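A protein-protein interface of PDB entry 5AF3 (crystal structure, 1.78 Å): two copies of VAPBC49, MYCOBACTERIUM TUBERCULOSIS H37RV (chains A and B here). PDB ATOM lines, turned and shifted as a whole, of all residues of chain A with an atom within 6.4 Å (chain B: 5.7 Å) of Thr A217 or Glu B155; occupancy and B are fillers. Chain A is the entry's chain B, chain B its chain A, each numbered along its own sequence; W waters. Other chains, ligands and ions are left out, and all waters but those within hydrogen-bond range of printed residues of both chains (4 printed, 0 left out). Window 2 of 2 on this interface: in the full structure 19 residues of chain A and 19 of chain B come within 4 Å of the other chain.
The backbone NH (N) of Phe A218 is in hydrogen-bond range of the side-chain carboxylate (OE1) of Glu B155 (3.0 Å).
N of Gln A219 lies close to OG1 of Thr A217, at 3.5 Å. OG1 of Thr A217 is in hydrogen-bond range of N of Ala A220 (3.0 Å).
Among the printed residues, pairs that only touch across the chains: Leu A212 with Ile B156, Gly A215 with Lys B154, Thr A217 with Glu B155, Phe A218 with Ile B156, Phe A218 with His B159 and Arg A233 with His B159.
Of the printed residues of chain B, Gly A215 touches Lys B154 (3.6 Å). Of the printed residues of chain A, Lys B154 touches Gly A215. Printed residues of chain B within 4 Å of Phe A218: Glu B155 (3.0 Å), Ile B156 (3.99 Å) and His B159 (3.8 Å). Printed residues of chain A within 4 Å of His B159: Phe A218 (3.8 Å) and Arg A233 (3.6 Å). Of the printed residues of chain A, Ile B156 touches Leu A212 (3.5 Å) and Phe A218 (3.99 Å). Pro A211 touches none of the printed residues of chain B. Arg B147 touches none of the printed residues of chain A. The nearest residue of chain A that does not touch Glu B155 is Gln A219 (4.5 Å).
Of the 12 printed residues of chain A, 5 touch a printed residue of chain B. Printed residues of chain A that touch a printed residue of chain B: Leu A212, Gly A215, Thr A217, Phe A218 and Arg A233. Of the 9 printed residues of chain B, 4 touch a printed residue of chain A. Printed residues of chain B that touch a printed residue of chain A: Lys B154, Glu B155, Ile B156 and His B159. Hydrophobic or aromatic side chains of chain B within 4 Å of the printed part of chain A: Ile B156 and His B159.
No position is printed for both chains. Of the 7 pairs that touch across the chains among the printed residues, none has its exchanged pair printed and touching as well.
Water W2 lies within hydrogen-bond range of the backbone carbonyl oxygen of Gly A215 (2.8 Å) and the backbone NH of Glu B155 (2.8 Å). Water W3 lies within hydrogen-bond range of O of Ala A216 (2.8 Å), O of Leu A212 (2.8 Å), N of Ile B156 (3.0 Å) and N of Glu B155 (3.3 Å). Water W1 lies within hydrogen-bond range of OE1 of Glu B155, N of Gln A219 and N of Phe A218. Water W4 lies within hydrogen-bond range of the side-chain carboxylate of Glu B155 (3.1 Å) and the guanidinium group of Arg A233 (3.3 Å).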
ATOM      1  N   PRO A 211     -10.917  19.202 -12.502  1.00  0.00           N
ATOM      2  CA  PRO A 211      -9.608  19.852 -12.531  1.00  0.00           C
ATOM      3  C   PRO A 211      -8.392  18.889 -12.677  1.00  0.00           C
ATOM      4  O   PRO A 211      -7.487  19.155 -13.462  1.00  0.00           O
ATOM      5  CB  PRO A 211      -9.561  20.586 -11.188  1.00  0.00           C
ATOM      6  CG  PRO A 211     -10.975  20.755 -10.792  1.00  0.00           C
ATOM      7  CD  PRO A 211     -11.713  19.612 -11.327  1.00  0.00           C
ATOM      8  N   LEU A 212      -8.385  17.771 -11.945  1.00  0.00           N
ATOM      9  CA  LEU A 212      -7.320  16.778 -12.114  1.00  0.00           C
ATOM     10  C   LEU A 212      -7.337  16.160 -13.505  1.00  0.00           C
ATOM     11  O   LEU A 212      -6.284  16.073 -14.165  1.00  0.00           O
ATOM     12  CB  LEU A 212      -7.426  15.688 -11.057  1.00  0.00           C
ATOM     13  CG  LEU A 212      -7.096  16.087  -9.637  1.00  0.00           C
ATOM     14  CD1 LEU A 212      -7.419  14.952  -8.679  1.00  0.00           C
ATOM     15  CD2 LEU A 212      -5.584  16.506  -9.507  1.00  0.00           C
ATOM     16  N   GLY A 215      -5.717  18.165 -16.107  1.00  0.00           N
ATOM     17  CA  GLY A 215      -4.286  18.267 -16.079  1.00  0.00           C
ATOM     18  C   GLY A 215      -3.698  19.201 -15.060  1.00  0.00           C
ATOM     19  O   GLY A 215      -2.477  19.419 -15.057  1.00  0.00           O
ATOM     20  N   ALA A 216      -4.526  19.763 -14.174  1.00  0.00           N
ATOM     21  CA  ALA A 216      -3.971  20.436 -12.992  1.00  0.00           C
ATOM     22  C   ALA A 216      -3.151  19.489 -12.110  1.00  0.00           C
ATOM     23  O   ALA A 216      -3.400  18.262 -12.071  1.00  0.00           O
ATOM     24  CB  ALA A 216      -5.078  21.157 -12.154  1.00  0.00           C
ATOM     25  N   THR A 217      -2.141  20.047 -11.441  1.00  0.00           N
ATOM     26  CA  THR A 217      -1.289  19.236 -10.577  1.00  0.00           C
ATOM     27  C   THR A 217      -2.052  18.926  -9.286  1.00  0.00           C
ATOM     28  O   THR A 217      -3.007  19.652  -8.927  1.00  0.00           O
ATOM     29  CB  THR A 217       0.009  19.953 -10.229  1.00  0.00           C
ATOM     30  OG1 THR A 217      -0.297  21.063  -9.367  1.00  0.00           O
ATOM     31  CG2 THR A 217       0.704  20.428 -11.504  1.00  0.00           C
ATOM     32  N   PHE A 218      -1.649  17.855  -8.600  1.00  0.00           N
ATOM     33  CA  PHE A 218      -2.217  17.553  -7.289  1.00  0.00           C
ATOM     34  C   PHE A 218      -2.043  18.739  -6.325  1.00  0.00           C
ATOM     35  O   PHE A 218      -2.940  19.046  -5.560  1.00  0.00           O
ATOM     36  CB  PHE A 218      -1.640  16.258  -6.688  1.00  0.00           C
ATOM     37  CG  PHE A 218      -2.229  15.017  -7.291  1.00  0.00           C
ATOM     38  CD1 PHE A 218      -3.448  14.516  -6.840  1.00  0.00           C
ATOM     39  CD2 PHE A 218      -1.566  14.355  -8.327  1.00  0.00           C
ATOM     40  CE1 PHE A 218      -4.011  13.332  -7.404  1.00  0.00           C
ATOM     41  CE2 PHE A 218      -2.116  13.212  -8.922  1.00  0.00           C
ATOM     42  CZ  PHE A 218      -3.339  12.690  -8.451  1.00  0.00           C
ATOM     43  N   GLN A 219      -0.889  19.406  -6.367  1.00  0.00           N
ATOM     44  CA  GLN A 219      -0.662  20.554  -5.476  1.00  0.00           C
ATOM     45  C   GLN A 219      -1.643  21.709  -5.747  1.00  0.00           C
ATOM     46  O   GLN A 219      -2.205  22.284  -4.789  1.00  0.00           O
ATOM     47  CB  GLN A 219       0.818  21.042  -5.542  1.00  0.00           C
ATOM     48  CG  GLN A 219       1.176  22.096  -4.485  1.00  0.00           C
ATOM     49  CD  GLN A 219       0.967  21.562  -3.098  1.00  0.00           C
ATOM     50  OE1 GLN A 219       0.056  21.997  -2.376  1.00  0.00           O
ATOM     51  NE2 GLN A 219       1.783  20.582  -2.711  1.00  0.00           N
ATOM     52  N   ALA A 220      -1.838  22.035  -7.025  1.00  0.00           N
ATOM     53  CA  ALA A 220      -2.698  23.158  -7.439  1.00  0.00           C
ATOM     54  C   ALA A 220      -4.137  22.862  -7.047  1.00  0.00           C
ATOM     55  O   ALA A 220      -4.821  23.715  -6.499  1.00  0.00           O
ATOM     56  CB  ALA A 220      -2.603  23.435  -8.931  1.00  0.00           C
ATOM     57  N   VAL A 221      -4.579  21.633  -7.307  1.00  0.00           N
ATOM     58  CA  VAL A 221      -5.966  21.243  -6.951  1.00  0.00           C
ATOM     59  C   VAL A 221      -6.171  21.280  -5.433  1.00  0.00           C
ATOM     60  O   VAL A 221      -7.164  21.833  -4.971  1.00  0.00           O
ATOM     61  CB  VAL A 221      -6.371  19.870  -7.565  1.00  0.00           C
ATOM     62  CG1 VAL A 221      -7.799  19.476  -7.129  1.00  0.00           C
ATOM     63  CG2 VAL A 221      -6.318  19.970  -9.106  1.00  0.00           C
ATOM     64  N   ALA A 222      -5.222  20.723  -4.680  1.00  0.00           N
ATOM     65  CA  ALA A 222      -5.316  20.617  -3.219  1.00  0.00           C
ATOM     66  C   ALA A 222      -5.438  21.996  -2.597  1.00  0.00           C
ATOM     67  O   ALA A 222      -6.273  22.219  -1.714  1.00  0.00           O
ATOM     68  CB  ALA A 222      -4.105  19.895  -2.657  1.00  0.00           C
ATOM     69  N   LEU A 232      -6.103  14.098  -1.725  1.00  0.00           N
ATOM     70  CA  LEU A 232      -6.626  13.992  -3.092  1.00  0.00           C
ATOM     71  C   LEU A 232      -6.347  12.623  -3.690  1.00  0.00           C
ATOM     72  O   LEU A 232      -7.217  12.065  -4.361  1.00  0.00           O
ATOM     73  CB  LEU A 232      -6.015  15.034  -4.021  1.00  0.00           C
ATOM     74  CG  LEU A 232      -6.576  16.417  -4.099  1.00  0.00           C
ATOM     75  CD1 LEU A 232      -5.731  17.199  -5.127  1.00  0.00           C
ATOM     76  CD2 LEU A 232      -8.073  16.346  -4.461  1.00  0.00           C
ATOM     77  N   ARG A 233      -5.123  12.114  -3.471  1.00  0.00           N
ATOM     78  CA  ARG A 233      -4.772  10.777  -3.979  1.00  0.00           C
ATOM     79  C   ARG A 233      -5.674   9.724  -3.358  1.00  0.00           C
ATOM     80  O   ARG A 233      -6.203   8.841  -4.073  1.00  0.00           O
ATOM     81  CB  ARG A 233      -3.302  10.429  -3.750  1.00  0.00           C
ATOM     82  CG  ARG A 233      -2.354  11.114  -4.730  1.00  0.00           C
ATOM     83  CD  ARG A 233      -0.890  11.064  -4.197  1.00  0.00           C
ATOM     84  NE  ARG A 233      -0.115  12.126  -4.809  1.00  0.00           N
ATOM     85  CZ  ARG A 233       0.399  13.171  -4.171  1.00  0.00           C
ATOM     86  NH1 ARG A 233       0.296  13.312  -2.854  1.00  0.00           N
ATOM     87  NH2 ARG A 233       1.061  14.065  -4.868  1.00  0.00           N
ATOM     88  N   ARG B 147       4.214  21.836 -19.395  1.00  0.00           N
ATOM     89  CA  ARG B 147       4.785  22.220 -18.118  1.00  0.00           C
ATOM     90  C   ARG B 147       6.171  22.796 -18.377  1.00  0.00           C
ATOM     91  O   ARG B 147       7.007  22.130 -18.987  1.00  0.00           O
ATOM     92  CB  ARG B 147       4.874  21.023 -17.182  1.00  0.00           C
ATOM     93  CG  ARG B 147       5.109  21.403 -15.742  1.00  0.00           C
ATOM     94  CD  ARG B 147       5.643  20.236 -14.942  1.00  0.00           C
ATOM     95  NE  ARG B 147       6.669  20.683 -14.004  1.00  0.00           N
ATOM     96  CZ  ARG B 147       6.425  21.264 -12.830  1.00  0.00           C
ATOM     97  NH1 ARG B 147       5.172  21.469 -12.422  1.00  0.00           N
ATOM     98  NH2 ARG B 147       7.442  21.636 -12.059  1.00  0.00           N
ATOM     99  N   PHE B 153       3.226  14.136 -19.026  1.00  0.00           N
ATOM    100  CA  PHE B 153       1.975  13.486 -18.617  1.00  0.00           C
ATOM    101  C   PHE B 153       1.289  14.281 -17.505  1.00  0.00           C
ATOM    102  O   PHE B 153       1.950  14.817 -16.624  1.00  0.00           O
ATOM    103  CB  PHE B 153       2.226  12.082 -18.086  1.00  0.00           C
ATOM    104  CG  PHE B 153       2.402  11.049 -19.152  1.00  0.00           C
ATOM    105  CD1 PHE B 153       1.366  10.728 -20.033  1.00  0.00           C
ATOM    106  CD2 PHE B 153       3.625  10.342 -19.239  1.00  0.00           C
ATOM    107  CE1 PHE B 153       1.528   9.733 -21.016  1.00  0.00           C
ATOM    108  CE2 PHE B 153       3.795   9.329 -20.200  1.00  0.00           C
ATOM    109  CZ  PHE B 153       2.776   9.020 -21.095  1.00  0.00           C
ATOM    110  N   LYS B 154      -0.045  14.398 -17.588  1.00  0.00           N
ATOM    111  CA  LYS B 154      -0.826  14.931 -16.475  1.00  0.00           C
ATOM    112  C   LYS B 154      -0.509  14.124 -15.212  1.00  0.00           C
ATOM    113  O   LYS B 154      -0.319  12.899 -15.276  1.00  0.00           O
ATOM    114  CB  LYS B 154      -2.313  14.761 -16.788  1.00  0.00           C
ATOM    115  CG  LYS B 154      -2.805  15.599 -17.968  1.00  0.00           C
ATOM    116  CD  LYS B 154      -4.274  15.333 -18.214  1.00  0.00           C
ATOM    117  CE  LYS B 154      -4.747  16.152 -19.405  1.00  0.00           C
ATOM    118  NZ  LYS B 154      -6.138  15.753 -19.782  1.00  0.00           N
ATOM    119  N   GLU B 155      -0.445  14.801 -14.070  1.00  0.00           N
ATOM    120  CA  GLU B 155      -0.170  14.116 -12.797  1.00  0.00           C
ATOM    121  C   GLU B 155      -1.183  13.055 -12.456  1.00  0.00           C
ATOM    122  O   GLU B 155      -0.835  12.055 -11.827  1.00  0.00           O
ATOM    123  CB  GLU B 155      -0.046  15.123 -11.649  1.00  0.00           C
ATOM    124  CG  GLU B 155       1.284  15.893 -11.760  1.00  0.00           C
ATOM    125  CD  GLU B 155       1.659  16.658 -10.496  1.00  0.00           C
ATOM    126  OE1 GLU B 155       0.884  16.638  -9.509  1.00  0.00           O
ATOM    127  OE2 GLU B 155       2.755  17.277 -10.492  1.00  0.00           O
ATOM    128  N   ILE B 156      -2.427  13.233 -12.899  1.00  0.00           N
ATOM    129  CA  ILE B 156      -3.456  12.225 -12.636  1.00  0.00           C
ATOM    130  C   ILE B 156      -3.088  10.882 -13.299  1.00  0.00           C
ATOM    131  O   ILE B 156      -3.428   9.821 -12.790  1.00  0.00           O
ATOM    132  CB  ILE B 156      -4.892  12.697 -13.074  1.00  0.00           C
ATOM    133  CG1 ILE B 156      -5.973  11.721 -12.553  1.00  0.00           C
ATOM    134  CG2 ILE B 156      -5.046  12.853 -14.632  1.00  0.00           C
ATOM    135  CD1 ILE B 156      -7.437  12.147 -12.945  1.00  0.00           C
ATOM    136  N   VAL B 157      -2.363  10.941 -14.418  1.00  0.00           N
ATOM    137  CA  VAL B 157      -1.808   9.734 -15.085  1.00  0.00           C
ATOM    138  C   VAL B 157      -0.504   9.295 -14.374  1.00  0.00           C
ATOM    139  O   VAL B 157      -0.345   8.089 -14.052  1.00  0.00           O
ATOM    140  CB  VAL B 157      -1.541   9.992 -16.606  1.00  0.00           C
ATOM    141  CG1 VAL B 157      -0.947   8.713 -17.291  1.00  0.00           C
ATOM    142  CG2 VAL B 157      -2.836  10.363 -17.314  1.00  0.00           C
ATOM    143  N   GLU B 158       0.415  10.239 -14.171  1.00  0.00           N
ATOM    144  CA  GLU B 158       1.705   9.945 -13.487  1.00  0.00           C
ATOM    145  C   GLU B 158       1.513   9.210 -12.171  1.00  0.00           C
ATOM    146  O   GLU B 158       2.232   8.236 -11.890  1.00  0.00           O
ATOM    147  CB  GLU B 158       2.485  11.212 -13.187  1.00  0.00           C
ATOM    148  CG  GLU B 158       3.306  11.708 -14.307  1.00  0.00           C
ATOM    149  CD  GLU B 158       4.280  12.787 -13.858  1.00  0.00           C
ATOM    150  OE1 GLU B 158       4.073  13.414 -12.784  1.00  0.00           O
ATOM    151  OE2 GLU B 158       5.244  13.014 -14.606  1.00  0.00           O
ATOM    152  N   HIS B 159       0.558   9.667 -11.363  1.00  0.00           N
ATOM    153  CA  HIS B 159       0.241   8.983 -10.071  1.00  0.00           C
ATOM    154  C   HIS B 159       0.099   7.463 -10.227  1.00  0.00           C
ATOM    155  O   HIS B 159       0.629   6.682  -9.406  1.00  0.00           O
ATOM    156  CB  HIS B 159      -1.014   9.612  -9.434  1.00  0.00           C
ATOM    157  CG  HIS B 159      -1.611   8.834  -8.290  1.00  0.00           C
ATOM    158  ND1 HIS B 159      -0.928   8.571  -7.120  1.00  0.00           N
ATOM    159  CD2 HIS B 159      -2.838   8.278  -8.143  1.00  0.00           C
ATOM    160  CE1 HIS B 159      -1.711   7.896  -6.296  1.00  0.00           C
ATOM    161  NE2 HIS B 159      -2.877   7.709  -6.890  1.00  0.00           N
ATOM    162  N   TYR B 160      -0.593   7.014 -11.263  1.00  0.00           N
ATOM    163  CA  TYR B 160      -0.678   5.577 -11.480  1.00  0.00           C
ATOM    164  C   TYR B 160       0.595   4.932 -12.051  1.00  0.00           C
ATOM    165  O   TYR B 160       0.933   3.806 -11.679  1.00  0.00           O
ATOM    166  CB  TYR B 160      -1.905   5.229 -12.311  1.00  0.00           C
ATOM    167  CG  TYR B 160      -3.127   5.646 -11.522  1.00  0.00           C
ATOM    168  CD1 TYR B 160      -3.622   4.826 -10.518  1.00  0.00           C
ATOM    169  CD2 TYR B 160      -3.719   6.899 -11.719  1.00  0.00           C
ATOM    170  CE1 TYR B 160      -4.699   5.242  -9.722  1.00  0.00           C
ATOM    171  CE2 TYR B 160      -4.794   7.331 -10.935  1.00  0.00           C
ATOM    172  CZ  TYR B 160      -5.278   6.498  -9.944  1.00  0.00           C
ATOM    173  OH  TYR B 160      -6.342   6.887  -9.147  1.00  0.00           O
HETATM  174  O   HOH W   1       1.516  18.237  -7.317  1.00  0.00           O
HETATM  175  O   HOH W   2      -0.603  17.598 -14.142  1.00  0.00           O
HETATM  176  O   HOH W   3      -3.527  15.909 -13.545  1.00  0.00           O
HETATM  177  O   HOH W   4       2.034  14.240  -7.968  1.00  0.00           O
